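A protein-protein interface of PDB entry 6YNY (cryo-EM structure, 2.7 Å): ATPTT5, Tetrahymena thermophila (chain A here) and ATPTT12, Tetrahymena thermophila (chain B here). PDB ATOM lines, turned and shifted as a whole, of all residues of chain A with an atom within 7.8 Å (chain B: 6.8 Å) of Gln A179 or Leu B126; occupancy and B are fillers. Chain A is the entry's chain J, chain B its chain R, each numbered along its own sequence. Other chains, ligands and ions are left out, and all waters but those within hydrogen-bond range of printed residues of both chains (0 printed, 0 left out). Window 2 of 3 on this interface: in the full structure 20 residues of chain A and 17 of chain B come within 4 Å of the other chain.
The guanidinium group of Arg A168 is in hydrogen-bond range of the backbone carbonyl oxygen of Thr B118 (2.6 Å). O of Leu B126 is in hydrogen-bond range of NE2 of Gln A179 (3.1 Å).
Thr B118 touches Phe A169. Thr A171 touches Phe B128 (O to CE2, 3.5 Å). Thr B118 touches Lys A172. Lys A172 touches Leu B123. CD1 of Leu B126 touches CG of Lys A172, 3.4 Å away. Ala A175 touches Leu B126. Phe B128 touches Ala A175 (CE2 to CB, 3.7 Å).
Of the 9 printed residues of chain B, 4 touch a printed residue of chain A. Hydrophobic or aromatic side chains of chain B that line the printed part of chain A: Leu B123, Leu B126 and Phe B128. Of the 17 printed residues of chain A, 6 touch a printed residue of chain B. Hydrophobic or aromatic side chains of chain A that line the printed part of chain B: Ala A175.
Gln A179 touches just one residue of chain B: Leu B126. Leu B126 touches just these residues of chain A: Lys A172 (3.4 Å), Ala A175 (3.8 Å) and Gln A179 (3.1 Å). Of the printed residues of chain B, Arg A168 touches Thr B118 (2.6 Å). Of the printed residues of chain B, Ala A175 touches Leu B126 (3.8 Å) and Phe B128 (3.7 Å). The nearest residue of chain B that does not touch Gln A179 is Asp B125 (4.4 Å). The nearest residue of chain A that does not touch Leu B126 is Ile A176 (4.1 Å). The nearest printed residue of chain B that does not touch Thr A171 is Leu B123 (4.3 Å).
O of Leu B123 lies within hydrogen-bond range of N of Phe B128, 2.9 Å away.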
ATOM      1  N   ARG A 168      21.590  24.691   0.999  1.00  0.00           N
ATOM      2  CA  ARG A 168      20.573  25.411   0.248  1.00  0.00           C
ATOM      3  C   ARG A 168      19.376  24.525  -0.061  1.00  0.00           C
ATOM      4  O   ARG A 168      18.239  25.008  -0.079  1.00  0.00           O
ATOM      5  CB  ARG A 168      21.185  25.964  -1.033  1.00  0.00           C
ATOM      6  CG  ARG A 168      22.235  27.017  -0.780  1.00  0.00           C
ATOM      7  CD  ARG A 168      23.029  27.334  -2.019  1.00  0.00           C
ATOM      8  NE  ARG A 168      22.189  27.740  -3.137  1.00  0.00           N
ATOM      9  CZ  ARG A 168      21.675  28.956  -3.286  1.00  0.00           C
ATOM     10  NH1 ARG A 168      21.905  29.900  -2.385  1.00  0.00           N
ATOM     11  NH2 ARG A 168      20.928  29.226  -4.343  1.00  0.00           N
ATOM     12  N   PHE A 169      19.605  23.234  -0.297  1.00  0.00           N
ATOM     13  CA  PHE A 169      18.496  22.315  -0.520  1.00  0.00           C
ATOM     14  C   PHE A 169      17.659  22.155   0.740  1.00  0.00           C
ATOM     15  O   PHE A 169      16.443  22.381   0.727  1.00  0.00           O
ATOM     16  CB  PHE A 169      19.018  20.957  -0.982  1.00  0.00           C
ATOM     17  CG  PHE A 169      18.046  19.844  -0.765  1.00  0.00           C
ATOM     18  CD1 PHE A 169      16.948  19.697  -1.586  1.00  0.00           C
ATOM     19  CD2 PHE A 169      18.220  18.951   0.271  1.00  0.00           C
ATOM     20  CE1 PHE A 169      16.052  18.684  -1.381  1.00  0.00           C
ATOM     21  CE2 PHE A 169      17.324  17.936   0.479  1.00  0.00           C
ATOM     22  CZ  PHE A 169      16.238  17.802  -0.348  1.00  0.00           C
ATOM     23  N   THR A 171      17.487  24.028   3.191  1.00  0.00           N
ATOM     24  CA  THR A 171      16.809  25.297   3.424  1.00  0.00           C
ATOM     25  C   THR A 171      15.564  25.416   2.560  1.00  0.00           C
ATOM     26  O   THR A 171      14.542  25.954   3.000  1.00  0.00           O
ATOM     27  CB  THR A 171      17.765  26.452   3.142  1.00  0.00           C
ATOM     28  OG1 THR A 171      18.888  26.372   4.024  1.00  0.00           O
ATOM     29  CG2 THR A 171      17.069  27.778   3.324  1.00  0.00           C
ATOM     30  N   LYS A 172      15.632  24.915   1.329  1.00  0.00           N
ATOM     31  CA  LYS A 172      14.464  24.913   0.458  1.00  0.00           C
ATOM     32  C   LYS A 172      13.408  23.941   0.963  1.00  0.00           C
ATOM     33  O   LYS A 172      12.227  24.290   1.069  1.00  0.00           O
ATOM     34  CB  LYS A 172      14.891  24.557  -0.962  1.00  0.00           C
ATOM     35  CG  LYS A 172      13.810  24.690  -1.999  1.00  0.00           C
ATOM     36  CD  LYS A 172      13.809  23.514  -2.943  1.00  0.00           C
ATOM     37  CE  LYS A 172      15.107  23.390  -3.690  1.00  0.00           C
ATOM     38  NZ  LYS A 172      15.085  22.245  -4.625  1.00  0.00           N
ATOM     39  N   ALA A 173      13.817  22.711   1.279  1.00  0.00           N
ATOM     40  CA  ALA A 173      12.874  21.731   1.800  1.00  0.00           C
ATOM     41  C   ALA A 173      12.285  22.174   3.128  1.00  0.00           C
ATOM     42  O   ALA A 173      11.119  21.890   3.417  1.00  0.00           O
ATOM     43  CB  ALA A 173      13.567  20.379   1.951  1.00  0.00           C
ATOM     44  N   LEU A 174      13.075  22.866   3.946  1.00  0.00           N
ATOM     45  CA  LEU A 174      12.566  23.382   5.210  1.00  0.00           C
ATOM     46  C   LEU A 174      11.397  24.329   4.984  1.00  0.00           C
ATOM     47  O   LEU A 174      10.410  24.301   5.727  1.00  0.00           O
ATOM     48  CB  LEU A 174      13.690  24.087   5.961  1.00  0.00           C
ATOM     49  CG  LEU A 174      13.332  24.768   7.275  1.00  0.00           C
ATOM     50  CD1 LEU A 174      12.801  23.765   8.261  1.00  0.00           C
ATOM     51  CD2 LEU A 174      14.542  25.471   7.827  1.00  0.00           C
ATOM     52  N   ALA A 175      11.491  25.179   3.962  1.00  0.00           N
ATOM     53  CA  ALA A 175      10.400  26.096   3.663  1.00  0.00           C
ATOM     54  C   ALA A 175       9.216  25.367   3.046  1.00  0.00           C
ATOM     55  O   ALA A 175       8.060  25.665   3.367  1.00  0.00           O
ATOM     56  CB  ALA A 175      10.891  27.194   2.726  1.00  0.00           C
ATOM     57  N   ILE A 176       9.481  24.409   2.158  1.00  0.00           N
ATOM     58  CA  ILE A 176       8.399  23.676   1.513  1.00  0.00           C
ATOM     59  C   ILE A 176       7.610  22.869   2.530  1.00  0.00           C
ATOM     60  O   ILE A 176       6.406  22.646   2.358  1.00  0.00           O
ATOM     61  CB  ILE A 176       8.969  22.789   0.393  1.00  0.00           C
ATOM     62  CG1 ILE A 176       9.517  23.671  -0.726  1.00  0.00           C
ATOM     63  CG2 ILE A 176       7.911  21.844  -0.119  1.00  0.00           C
ATOM     64  CD1 ILE A 176      10.320  22.949  -1.756  1.00  0.00           C
ATOM     65  N   ASN A 177       8.261  22.418   3.601  1.00  0.00           N
ATOM     66  CA  ASN A 177       7.555  21.684   4.641  1.00  0.00           C
ATOM     67  C   ASN A 177       6.758  22.608   5.551  1.00  0.00           C
ATOM     68  O   ASN A 177       5.695  22.217   6.042  1.00  0.00           O
ATOM     69  CB  ASN A 177       8.541  20.859   5.465  1.00  0.00           C
ATOM     70  CG  ASN A 177       9.099  19.685   4.700  1.00  0.00           C
ATOM     71  OD1 ASN A 177       8.423  19.102   3.854  1.00  0.00           O
ATOM     72  ND2 ASN A 177      10.340  19.327   4.991  1.00  0.00           N
ATOM     73  N   ASN A 178       7.247  23.827   5.786  1.00  0.00           N
ATOM     74  CA  ASN A 178       6.530  24.759   6.645  1.00  0.00           C
ATOM     75  C   ASN A 178       5.361  25.418   5.927  1.00  0.00           C
ATOM     76  O   ASN A 178       4.380  25.797   6.574  1.00  0.00           O
ATOM     77  CB  ASN A 178       7.482  25.825   7.186  1.00  0.00           C
ATOM     78  CG  ASN A 178       8.261  25.351   8.389  1.00  0.00           C
ATOM     79  OD1 ASN A 178       7.809  25.478   9.524  1.00  0.00           O
ATOM     80  ND2 ASN A 178       9.440  24.805   8.151  1.00  0.00           N
ATOM     81  N   GLN A 179       5.444  25.575   4.606  1.00  0.00           N
ATOM     82  CA  GLN A 179       4.297  26.078   3.862  1.00  0.00           C
ATOM     83  C   GLN A 179       3.148  25.082   3.901  1.00  0.00           C
ATOM     84  O   GLN A 179       1.984  25.471   4.044  1.00  0.00           O
ATOM     85  CB  GLN A 179       4.692  26.379   2.421  1.00  0.00           C
ATOM     86  CG  GLN A 179       5.625  27.550   2.268  1.00  0.00           C
ATOM     87  CD  GLN A 179       5.870  27.903   0.822  1.00  0.00           C
ATOM     88  OE1 GLN A 179       5.336  27.267  -0.085  1.00  0.00           O
ATOM     89  NE2 GLN A 179       6.680  28.925   0.596  1.00  0.00           N
ATOM     90  N   THR A 180       3.459  23.793   3.770  1.00  0.00           N
ATOM     91  CA  THR A 180       2.440  22.766   3.937  1.00  0.00           C
ATOM     92  C   THR A 180       1.876  22.788   5.349  1.00  0.00           C
ATOM     93  O   THR A 180       0.672  22.589   5.551  1.00  0.00           O
ATOM     94  CB  THR A 180       3.035  21.397   3.615  1.00  0.00           C
ATOM     95  OG1 THR A 180       3.602  21.416   2.301  1.00  0.00           O
ATOM     96  CG2 THR A 180       1.983  20.322   3.686  1.00  0.00           C
ATOM     97  N   TYR A 181       2.733  23.034   6.340  1.00  0.00           N
ATOM     98  CA  TYR A 181       2.271  23.181   7.715  1.00  0.00           C
ATOM     99  C   TYR A 181       1.252  24.304   7.834  1.00  0.00           C
ATOM    100  O   TYR A 181       0.227  24.157   8.507  1.00  0.00           O
ATOM    101  CB  TYR A 181       3.468  23.448   8.622  1.00  0.00           C
ATOM    102  CG  TYR A 181       3.165  23.499  10.097  1.00  0.00           C
ATOM    103  CD1 TYR A 181       3.410  22.408  10.907  1.00  0.00           C
ATOM    104  CD2 TYR A 181       2.651  24.642  10.683  1.00  0.00           C
ATOM    105  CE1 TYR A 181       3.148  22.448  12.251  1.00  0.00           C
ATOM    106  CE2 TYR A 181       2.384  24.692  12.029  1.00  0.00           C
ATOM    107  CZ  TYR A 181       2.632  23.591  12.809  1.00  0.00           C
ATOM    108  OH  TYR A 181       2.370  23.628  14.156  1.00  0.00           O
ATOM    109  N   ILE A 182       1.515  25.433   7.177  1.00  0.00           N
ATOM    110  CA  ILE A 182       0.623  26.582   7.272  1.00  0.00           C
ATOM    111  C   ILE A 182      -0.707  26.285   6.596  1.00  0.00           C
ATOM    112  O   ILE A 182      -1.774  26.597   7.134  1.00  0.00           O
ATOM    113  CB  ILE A 182       1.310  27.819   6.673  1.00  0.00           C
ATOM    114  CG1 ILE A 182       2.506  28.210   7.538  1.00  0.00           C
ATOM    115  CG2 ILE A 182       0.342  28.973   6.563  1.00  0.00           C
ATOM    116  CD1 ILE A 182       3.481  29.113   6.857  1.00  0.00           C
ATOM    117  N   ARG A 183      -0.671  25.682   5.407  1.00  0.00           N
ATOM    118  CA  ARG A 183      -1.913  25.319   4.739  1.00  0.00           C
ATOM    119  C   ARG A 183      -2.672  24.259   5.519  1.00  0.00           C
ATOM    120  O   ARG A 183      -3.908  24.256   5.524  1.00  0.00           O
ATOM    121  CB  ARG A 183      -1.628  24.818   3.325  1.00  0.00           C
ATOM    122  CG  ARG A 183      -0.942  25.825   2.432  1.00  0.00           C
ATOM    123  CD  ARG A 183      -0.979  25.374   0.992  1.00  0.00           C
ATOM    124  NE  ARG A 183      -0.460  24.020   0.834  1.00  0.00           N
ATOM    125  CZ  ARG A 183       0.803  23.726   0.545  1.00  0.00           C
ATOM    126  NH1 ARG A 183       1.699  24.688   0.377  1.00  0.00           N
ATOM    127  NH2 ARG A 183       1.173  22.460   0.425  1.00  0.00           N
ATOM    128  N   ALA A 184      -1.952  23.360   6.187  1.00  0.00           N
ATOM    129  CA  ALA A 184      -2.601  22.288   6.926  1.00  0.00           C
ATOM    130  C   ALA A 184      -3.231  22.798   8.212  1.00  0.00           C
ATOM    131  O   ALA A 184      -4.354  22.414   8.555  1.00  0.00           O
ATOM    132  CB  ALA A 184      -1.589  21.191   7.233  1.00  0.00           C
ATOM    133  N   MET A 185      -2.527  23.661   8.934  1.00  0.00           N
ATOM    134  CA  MET A 185      -3.007  24.186  10.201  1.00  0.00           C
ATOM    135  C   MET A 185      -3.926  25.383  10.032  1.00  0.00           C
ATOM    136  O   MET A 185      -4.294  26.011  11.028  1.00  0.00           O
ATOM    137  CB  MET A 185      -1.821  24.563  11.087  1.00  0.00           C
ATOM    138  CG  MET A 185      -0.885  23.407  11.363  1.00  0.00           C
ATOM    139  SD  MET A 185      -1.669  22.055  12.249  1.00  0.00           S
ATOM    140  CE  MET A 185      -1.953  22.836  13.827  1.00  0.00           C
ATOM    141  N   THR B 118      20.068  24.560  -6.272  1.00  0.00           N
ATOM    142  CA  THR B 118      18.969  25.377  -5.782  1.00  0.00           C
ATOM    143  C   THR B 118      19.145  26.824  -6.221  1.00  0.00           C
ATOM    144  O   THR B 118      20.224  27.405  -6.080  1.00  0.00           O
ATOM    145  CB  THR B 118      18.891  25.289  -4.260  1.00  0.00           C
ATOM    146  OG1 THR B 118      18.785  23.918  -3.864  1.00  0.00           O
ATOM    147  CG2 THR B 118      17.695  26.050  -3.748  1.00  0.00           C
ATOM    148  N   GLU B 121      16.434  32.751  -6.852  1.00  0.00           N
ATOM    149  CA  GLU B 121      15.129  33.319  -7.163  1.00  0.00           C
ATOM    150  C   GLU B 121      13.999  32.489  -6.574  1.00  0.00           C
ATOM    151  O   GLU B 121      12.916  33.018  -6.308  1.00  0.00           O
ATOM    152  CB  GLU B 121      14.948  33.423  -8.676  1.00  0.00           C
ATOM    153  CG  GLU B 121      15.926  34.343  -9.377  1.00  0.00           C
ATOM    154  CD  GLU B 121      17.275  33.694  -9.628  1.00  0.00           C
ATOM    155  OE1 GLU B 121      17.527  32.606  -9.070  1.00  0.00           O
ATOM    156  OE2 GLU B 121      18.081  34.267 -10.388  1.00  0.00           O
ATOM    157  N   HIS B 122      14.232  31.195  -6.362  1.00  0.00           N
ATOM    158  CA  HIS B 122      13.192  30.327  -5.826  1.00  0.00           C
ATOM    159  C   HIS B 122      13.115  30.426  -4.309  1.00  0.00           C
ATOM    160  O   HIS B 122      12.022  30.371  -3.737  1.00  0.00           O
ATOM    161  CB  HIS B 122      13.458  28.890  -6.263  1.00  0.00           C
ATOM    162  CG  HIS B 122      12.327  27.950  -5.991  1.00  0.00           C
ATOM    163  ND1 HIS B 122      11.034  28.376  -5.781  1.00  0.00           N
ATOM    164  CD2 HIS B 122      12.298  26.601  -5.898  1.00  0.00           C
ATOM    165  CE1 HIS B 122      10.258  27.329  -5.568  1.00  0.00           C
ATOM    166  NE2 HIS B 122      11.001  26.239  -5.633  1.00  0.00           N
ATOM    167  N   LEU B 123      14.260  30.578  -3.644  1.00  0.00           N
ATOM    168  CA  LEU B 123      14.258  30.724  -2.193  1.00  0.00           C
ATOM    169  C   LEU B 123      13.566  32.011  -1.769  1.00  0.00           C
ATOM    170  O   LEU B 123      12.857  32.039  -0.757  1.00  0.00           O
ATOM    171  CB  LEU B 123      15.688  30.691  -1.662  1.00  0.00           C
ATOM    172  CG  LEU B 123      16.376  29.331  -1.656  1.00  0.00           C
ATOM    173  CD1 LEU B 123      17.820  29.483  -1.253  1.00  0.00           C
ATOM    174  CD2 LEU B 123      15.665  28.384  -0.718  1.00  0.00           C
ATOM    175  N   VAL B 124      13.768  33.091  -2.523  1.00  0.00           N
ATOM    176  CA  VAL B 124      13.096  34.348  -2.212  1.00  0.00           C
ATOM    177  C   VAL B 124      11.588  34.160  -2.232  1.00  0.00           C
ATOM    178  O   VAL B 124      10.875  34.632  -1.340  1.00  0.00           O
ATOM    179  CB  VAL B 124      13.544  35.443  -3.195  1.00  0.00           C
ATOM    180  CG1 VAL B 124      12.727  36.697  -3.003  1.00  0.00           C
ATOM    181  CG2 VAL B 124      15.009  35.740  -3.012  1.00  0.00           C
ATOM    182  N   ASP B 125      11.077  33.464  -3.246  1.00  0.00           N
ATOM    183  CA  ASP B 125       9.648  33.214  -3.345  1.00  0.00           C
ATOM    184  C   ASP B 125       9.158  32.189  -2.334  1.00  0.00           C
ATOM    185  O   ASP B 125       7.945  32.079  -2.130  1.00  0.00           O
ATOM    186  CB  ASP B 125       9.300  32.753  -4.755  1.00  0.00           C
ATOM    187  CG  ASP B 125       9.451  33.859  -5.783  1.00  0.00           C
ATOM    188  OD1 ASP B 125       9.878  34.968  -5.404  1.00  0.00           O
ATOM    189  OD2 ASP B 125       9.137  33.621  -6.967  1.00  0.00           O
ATOM    190  N   LEU B 126      10.059  31.439  -1.708  1.00  0.00           N
ATOM    191  CA  LEU B 126       9.690  30.470  -0.690  1.00  0.00           C
ATOM    192  C   LEU B 126       9.700  31.049   0.715  1.00  0.00           C
ATOM    193  O   LEU B 126       9.207  30.394   1.639  1.00  0.00           O
ATOM    194  CB  LEU B 126      10.635  29.269  -0.742  1.00  0.00           C
ATOM    195  CG  LEU B 126      10.474  28.325  -1.930  1.00  0.00           C
ATOM    196  CD1 LEU B 126      11.587  27.306  -1.943  1.00  0.00           C
ATOM    197  CD2 LEU B 126       9.137  27.638  -1.880  1.00  0.00           C
ATOM    198  N   GLY B 127      10.247  32.248   0.903  1.00  0.00           N
ATOM    199  CA  GLY B 127      10.280  32.894   2.198  1.00  0.00           C
ATOM    200  C   GLY B 127      11.656  33.033   2.803  1.00  0.00           C
ATOM    201  O   GLY B 127      11.767  33.513   3.935  1.00  0.00           O
ATOM    202  N   PHE B 128      12.703  32.629   2.095  1.00  0.00           N
ATOM    203  CA  PHE B 128      14.077  32.719   2.573  1.00  0.00           C
ATOM    204  C   PHE B 128      14.867  33.577   1.597  1.00  0.00           C
ATOM    205  O   PHE B 128      15.077  33.181   0.446  1.00  0.00           O
ATOM    206  CB  PHE B 128      14.701  31.331   2.707  1.00  0.00           C
ATOM    207  CG  PHE B 128      14.291  30.589   3.944  1.00  0.00           C
ATOM    208  CD1 PHE B 128      14.336  31.195   5.182  1.00  0.00           C
ATOM    209  CD2 PHE B 128      13.867  29.279   3.867  1.00  0.00           C
ATOM    210  CE1 PHE B 128      13.967  30.512   6.313  1.00  0.00           C
ATOM    211  CE2 PHE B 128      13.495  28.593   4.999  1.00  0.00           C
ATOM    212  CZ  PHE B 128      13.546  29.209   6.221  1.00  0.00           C
